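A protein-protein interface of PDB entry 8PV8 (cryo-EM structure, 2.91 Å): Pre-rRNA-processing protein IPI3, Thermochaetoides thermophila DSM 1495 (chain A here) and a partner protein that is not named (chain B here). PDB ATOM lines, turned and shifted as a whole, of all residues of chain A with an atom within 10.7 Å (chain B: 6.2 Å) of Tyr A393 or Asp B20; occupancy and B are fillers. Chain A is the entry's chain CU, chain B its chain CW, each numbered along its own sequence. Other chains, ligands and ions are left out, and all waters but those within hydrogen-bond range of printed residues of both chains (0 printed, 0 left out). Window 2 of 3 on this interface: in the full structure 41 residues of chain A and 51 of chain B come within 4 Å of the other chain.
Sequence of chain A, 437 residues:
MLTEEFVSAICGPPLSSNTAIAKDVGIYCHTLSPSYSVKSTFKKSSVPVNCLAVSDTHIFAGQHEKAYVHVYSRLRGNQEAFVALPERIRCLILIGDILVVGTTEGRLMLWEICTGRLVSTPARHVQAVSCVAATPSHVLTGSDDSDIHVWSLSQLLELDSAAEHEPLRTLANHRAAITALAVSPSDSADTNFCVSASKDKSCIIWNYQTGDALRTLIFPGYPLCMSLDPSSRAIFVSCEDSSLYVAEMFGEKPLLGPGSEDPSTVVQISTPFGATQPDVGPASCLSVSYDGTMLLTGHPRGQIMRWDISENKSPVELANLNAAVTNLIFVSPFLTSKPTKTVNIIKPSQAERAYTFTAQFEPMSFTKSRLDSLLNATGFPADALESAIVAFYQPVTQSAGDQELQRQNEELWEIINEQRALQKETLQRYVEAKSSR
The side-chain hydroxyl (OH) of Tyr A393 lies within hydrogen-bond range of the backbone carbonyl oxygen (O) of Asp B20.
Among the printed residues, pairs that only touch across the chains: Ile A389 with Pro B23 (3.3 Å), Phe A392 with Ala B76 (3.5 Å), Tyr A393 with Pro B23 (3.6 Å) and Tyr A393 with Arg B24 (3.6 Å).
Tyr A393 touches just these residues of chain B: Asp B20 (2.5 Å), Pro B23 (3.6 Å) and Arg B24 (3.6 Å).
Of chain A, only Tyr A393 comes within 4 Å of Asp B20.
No residue of chain A comes within 4 Å of Val B19.
No residue of chain A comes within 4 Å of Ser B21.
Of the printed residues of chain B, Ile A389 touches Pro B23 (3.3 Å).
Of the printed residues of chain B, Phe A392 touches Ala B76.
Of the printed residues of chain A, Arg B24 touches Tyr A393 (3.6 Å).
Ser A387 touches none of the printed residues of chain B.
The nearest residue of chain B that does not touch Tyr A393 is Ser B21 (4.1 Å).
The nearest printed residue of chain B that does not touch Phe A392 is Pro B23 (4.6 Å).
Of the 10 printed residues of chain B, 4 touch a printed residue of chain A.
Among the printed residues, 5 pairs touch across the chains.
Among the printed residues, no Asp or Glu carboxylate lies within 4 Å of a Lys or Arg side-chain nitrogen of the other chain.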
ATOM      1  N   LEU A 385     -30.796 -23.248  18.123  1.00  0.00           N
ATOM      2  CA  LEU A 385     -29.618 -22.841  18.878  1.00  0.00           C
ATOM      3  C   LEU A 385     -28.337 -23.381  18.256  1.00  0.00           C
ATOM      4  O   LEU A 385     -27.353 -22.647  18.115  1.00  0.00           O
ATOM      5  CB  LEU A 385     -29.744 -23.302  20.328  1.00  0.00           C
ATOM      6  CG  LEU A 385     -28.661 -22.839  21.301  1.00  0.00           C
ATOM      7  CD1 LEU A 385     -28.712 -21.336  21.497  1.00  0.00           C
ATOM      8  CD2 LEU A 385     -28.826 -23.554  22.626  1.00  0.00           C
ATOM      9  N   GLU A 386     -28.330 -24.659  17.864  1.00  0.00           N
ATOM     10  CA  GLU A 386     -27.120 -25.222  17.271  1.00  0.00           C
ATOM     11  C   GLU A 386     -26.877 -24.662  15.873  1.00  0.00           C
ATOM     12  O   GLU A 386     -25.722 -24.477  15.468  1.00  0.00           O
ATOM     13  CB  GLU A 386     -27.180 -26.754  17.261  1.00  0.00           C
ATOM     14  CG  GLU A 386     -28.252 -27.374  16.385  1.00  0.00           C
ATOM     15  CD  GLU A 386     -28.283 -28.887  16.481  1.00  0.00           C
ATOM     16  OE1 GLU A 386     -27.479 -29.451  17.252  1.00  0.00           O
ATOM     17  OE2 GLU A 386     -29.117 -29.512  15.792  1.00  0.00           O
ATOM     18  N   SER A 387     -27.948 -24.349  15.133  1.00  0.00           N
ATOM     19  CA  SER A 387     -27.784 -23.674  13.849  1.00  0.00           C
ATOM     20  C   SER A 387     -27.186 -22.284  14.031  1.00  0.00           C
ATOM     21  O   SER A 387     -26.314 -21.868  13.256  1.00  0.00           O
ATOM     22  CB  SER A 387     -29.125 -23.589  13.124  1.00  0.00           C
ATOM     23  OG  SER A 387     -28.991 -22.898  11.894  1.00  0.00           O
ATOM     24  N   ALA A 388     -27.634 -21.558  15.061  1.00  0.00           N
ATOM     25  CA  ALA A 388     -27.070 -20.245  15.355  1.00  0.00           C
ATOM     26  C   ALA A 388     -25.604 -20.345  15.756  1.00  0.00           C
ATOM     27  O   ALA A 388     -24.789 -19.511  15.350  1.00  0.00           O
ATOM     28  CB  ALA A 388     -27.880 -19.561  16.456  1.00  0.00           C
ATOM     29  N   ILE A 389     -25.251 -21.363  16.547  1.00  0.00           N
ATOM     30  CA  ILE A 389     -23.859 -21.557  16.954  1.00  0.00           C
ATOM     31  C   ILE A 389     -22.979 -21.849  15.743  1.00  0.00           C
ATOM     32  O   ILE A 389     -21.890 -21.274  15.594  1.00  0.00           O
ATOM     33  CB  ILE A 389     -23.763 -22.677  18.007  1.00  0.00           C
ATOM     34  CG1 ILE A 389     -24.405 -22.236  19.321  1.00  0.00           C
ATOM     35  CG2 ILE A 389     -22.317 -23.069  18.255  1.00  0.00           C
ATOM     36  CD1 ILE A 389     -24.736 -23.385  20.242  1.00  0.00           C
ATOM     37  N   VAL A 390     -23.445 -22.729  14.850  1.00  0.00           N
ATOM     38  CA  VAL A 390     -22.670 -23.082  13.662  1.00  0.00           C
ATOM     39  C   VAL A 390     -22.508 -21.876  12.741  1.00  0.00           C
ATOM     40  O   VAL A 390     -21.410 -21.608  12.237  1.00  0.00           O
ATOM     41  CB  VAL A 390     -23.323 -24.275  12.938  1.00  0.00           C
ATOM     42  CG1 VAL A 390     -22.721 -24.471  11.555  1.00  0.00           C
ATOM     43  CG2 VAL A 390     -23.152 -25.541  13.760  1.00  0.00           C
ATOM     44  N   ALA A 391     -23.583 -21.110  12.534  1.00  0.00           N
ATOM     45  CA  ALA A 391     -23.494 -19.957  11.643  1.00  0.00           C
ATOM     46  C   ALA A 391     -22.703 -18.817  12.279  1.00  0.00           C
ATOM     47  O   ALA A 391     -22.170 -17.954  11.572  1.00  0.00           O
ATOM     48  CB  ALA A 391     -24.894 -19.495  11.244  1.00  0.00           C
ATOM     49  N   PHE A 392     -22.623 -18.790  13.613  1.00  0.00           N
ATOM     50  CA  PHE A 392     -21.702 -17.875  14.279  1.00  0.00           C
ATOM     51  C   PHE A 392     -20.262 -18.293  14.020  1.00  0.00           C
ATOM     52  O   PHE A 392     -19.407 -17.454  13.718  1.00  0.00           O
ATOM     53  CB  PHE A 392     -22.027 -17.832  15.782  1.00  0.00           C
ATOM     54  CG  PHE A 392     -21.182 -16.865  16.595  1.00  0.00           C
ATOM     55  CD1 PHE A 392     -19.897 -17.191  17.020  1.00  0.00           C
ATOM     56  CD2 PHE A 392     -21.693 -15.624  16.939  1.00  0.00           C
ATOM     57  CE1 PHE A 392     -19.146 -16.300  17.761  1.00  0.00           C
ATOM     58  CE2 PHE A 392     -20.945 -14.728  17.682  1.00  0.00           C
ATOM     59  CZ  PHE A 392     -19.671 -15.066  18.091  1.00  0.00           C
ATOM     60  N   TYR A 393     -19.979 -19.587  14.131  1.00  0.00           N
ATOM     61  CA  TYR A 393     -18.636 -20.098  13.887  1.00  0.00           C
ATOM     62  C   TYR A 393     -18.386 -20.292  12.396  1.00  0.00           C
ATOM     63  O   TYR A 393     -18.372 -19.330  11.628  1.00  0.00           O
ATOM     64  CB  TYR A 393     -18.425 -21.412  14.635  1.00  0.00           C
ATOM     65  CG  TYR A 393     -18.119 -21.236  16.103  1.00  0.00           C
ATOM     66  CD1 TYR A 393     -17.608 -20.039  16.588  1.00  0.00           C
ATOM     67  CD2 TYR A 393     -18.350 -22.264  17.006  1.00  0.00           C
ATOM     68  CE1 TYR A 393     -17.328 -19.874  17.931  1.00  0.00           C
ATOM     69  CE2 TYR A 393     -18.076 -22.107  18.350  1.00  0.00           C
ATOM     70  CZ  TYR A 393     -17.565 -20.912  18.807  1.00  0.00           C
ATOM     71  OH  TYR A 393     -17.290 -20.755  20.145  1.00  0.00           O
ATOM     72  N   PRO B  18     -13.486 -20.507  29.067  1.00  0.00           N
ATOM     73  CA  PRO B  18     -13.084 -19.361  28.242  1.00  0.00           C
ATOM     74  C   PRO B  18     -14.240 -18.797  27.424  1.00  0.00           C
ATOM     75  O   PRO B  18     -15.172 -19.510  27.029  1.00  0.00           O
ATOM     76  CB  PRO B  18     -11.978 -19.931  27.343  1.00  0.00           C
ATOM     77  CG  PRO B  18     -11.953 -21.405  27.586  1.00  0.00           C
ATOM     78  CD  PRO B  18     -12.574 -21.651  28.912  1.00  0.00           C
ATOM     79  N   VAL B  19     -14.148 -17.490  27.168  1.00  0.00           N
ATOM     80  CA  VAL B  19     -15.236 -16.740  26.546  1.00  0.00           C
ATOM     81  C   VAL B  19     -15.454 -17.192  25.104  1.00  0.00           C
ATOM     82  O   VAL B  19     -16.590 -17.234  24.617  1.00  0.00           O
ATOM     83  CB  VAL B  19     -14.956 -15.226  26.664  1.00  0.00           C
ATOM     84  CG1 VAL B  19     -13.613 -14.847  26.038  1.00  0.00           C
ATOM     85  CG2 VAL B  19     -16.080 -14.408  26.068  1.00  0.00           C
ATOM     86  N   ASP B  20     -14.378 -17.568  24.408  1.00  0.00           N
ATOM     87  CA  ASP B  20     -14.501 -18.004  23.023  1.00  0.00           C
ATOM     88  C   ASP B  20     -15.189 -19.356  22.888  1.00  0.00           C
ATOM     89  O   ASP B  20     -15.880 -19.580  21.889  1.00  0.00           O
ATOM     90  CB  ASP B  20     -13.123 -18.054  22.364  1.00  0.00           C
ATOM     91  CG  ASP B  20     -13.203 -18.231  20.862  1.00  0.00           C
ATOM     92  OD1 ASP B  20     -13.571 -17.261  20.168  1.00  0.00           O
ATOM     93  OD2 ASP B  20     -12.901 -19.341  20.375  1.00  0.00           O
ATOM     94  N   SER B  21     -15.023 -20.256  23.857  1.00  0.00           N
ATOM     95  CA  SER B  21     -15.688 -21.551  23.828  1.00  0.00           C
ATOM     96  C   SER B  21     -17.002 -21.559  24.594  1.00  0.00           C
ATOM     97  O   SER B  21     -17.667 -22.600  24.637  1.00  0.00           O
ATOM     98  CB  SER B  21     -14.767 -22.639  24.385  1.00  0.00           C
ATOM     99  OG  SER B  21     -14.400 -22.352  25.719  1.00  0.00           O
ATOM    100  N   LEU B  22     -17.380 -20.441  25.218  1.00  0.00           N
ATOM    101  CA  LEU B  22     -18.716 -20.289  25.800  1.00  0.00           C
ATOM    102  C   LEU B  22     -19.884 -20.537  24.831  1.00  0.00           C
ATOM    103  O   LEU B  22     -20.900 -21.098  25.274  1.00  0.00           O
ATOM    104  CB  LEU B  22     -18.858 -18.905  26.446  1.00  0.00           C
ATOM    105  CG  LEU B  22     -18.343 -18.768  27.877  1.00  0.00           C
ATOM    106  CD1 LEU B  22     -18.493 -17.337  28.363  1.00  0.00           C
ATOM    107  CD2 LEU B  22     -19.074 -19.730  28.798  1.00  0.00           C
ATOM    108  N   PRO B  23     -19.837 -20.123  23.543  1.00  0.00           N
ATOM    109  CA  PRO B  23     -20.937 -20.513  22.633  1.00  0.00           C
ATOM    110  C   PRO B  23     -21.144 -22.011  22.471  1.00  0.00           C
ATOM    111  O   PRO B  23     -22.279 -22.450  22.253  1.00  0.00           O
ATOM    112  CB  PRO B  23     -20.535 -19.856  21.308  1.00  0.00           C
ATOM    113  CG  PRO B  23     -19.804 -18.678  21.697  1.00  0.00           C
ATOM    114  CD  PRO B  23     -19.032 -19.046  22.927  1.00  0.00           C
ATOM    115  N   ARG B  24     -20.082 -22.813  22.565  1.00  0.00           N
ATOM    116  CA  ARG B  24     -20.257 -24.260  22.486  1.00  0.00           C
ATOM    117  C   ARG B  24     -20.937 -24.809  23.732  1.00  0.00           C
ATOM    118  O   ARG B  24     -21.654 -25.814  23.655  1.00  0.00           O
ATOM    119  CB  ARG B  24     -18.911 -24.944  22.265  1.00  0.00           C
ATOM    120  CG  ARG B  24     -18.212 -24.514  20.993  1.00  0.00           C
ATOM    121  CD  ARG B  24     -17.078 -25.455  20.641  1.00  0.00           C
ATOM    122  NE  ARG B  24     -16.202 -24.894  19.621  1.00  0.00           N
ATOM    123  CZ  ARG B  24     -15.113 -24.183  19.880  1.00  0.00           C
ATOM    124  NH1 ARG B  24     -14.734 -23.929  21.121  1.00  0.00           N
ATOM    125  NH2 ARG B  24     -14.386 -23.718  18.868  1.00  0.00           N
ATOM    126  N   SER B  74     -15.940  -9.190  23.426  1.00  0.00           N
ATOM    127  CA  SER B  74     -15.958 -10.463  22.724  1.00  0.00           C
ATOM    128  C   SER B  74     -17.322 -10.709  22.081  1.00  0.00           C
ATOM    129  O   SER B  74     -18.347 -10.689  22.783  1.00  0.00           O
ATOM    130  CB  SER B  74     -15.620 -11.602  23.686  1.00  0.00           C
ATOM    131  OG  SER B  74     -15.497 -12.834  22.997  1.00  0.00           O
ATOM    132  N   ALA B  76     -18.278 -13.603  21.001  1.00  0.00           N
ATOM    133  CA  ALA B  76     -18.707 -14.857  21.612  1.00  0.00           C
ATOM    134  C   ALA B  76     -19.348 -14.613  22.973  1.00  0.00           C
ATOM    135  O   ALA B  76     -20.364 -15.237  23.314  1.00  0.00           O
ATOM    136  CB  ALA B  76     -17.517 -15.805  21.738  1.00  0.00           C
ATOM    137  N   GLY B  77     -18.772 -13.697  23.754  1.00  0.00           N
ATOM    138  CA  GLY B  77     -19.384 -13.323  25.016  1.00  0.00           C
ATOM    139  C   GLY B  77     -20.724 -12.644  24.832  1.00  0.00           C
ATOM    140  O   GLY B  77     -21.646 -12.858  25.620  1.00  0.00           O
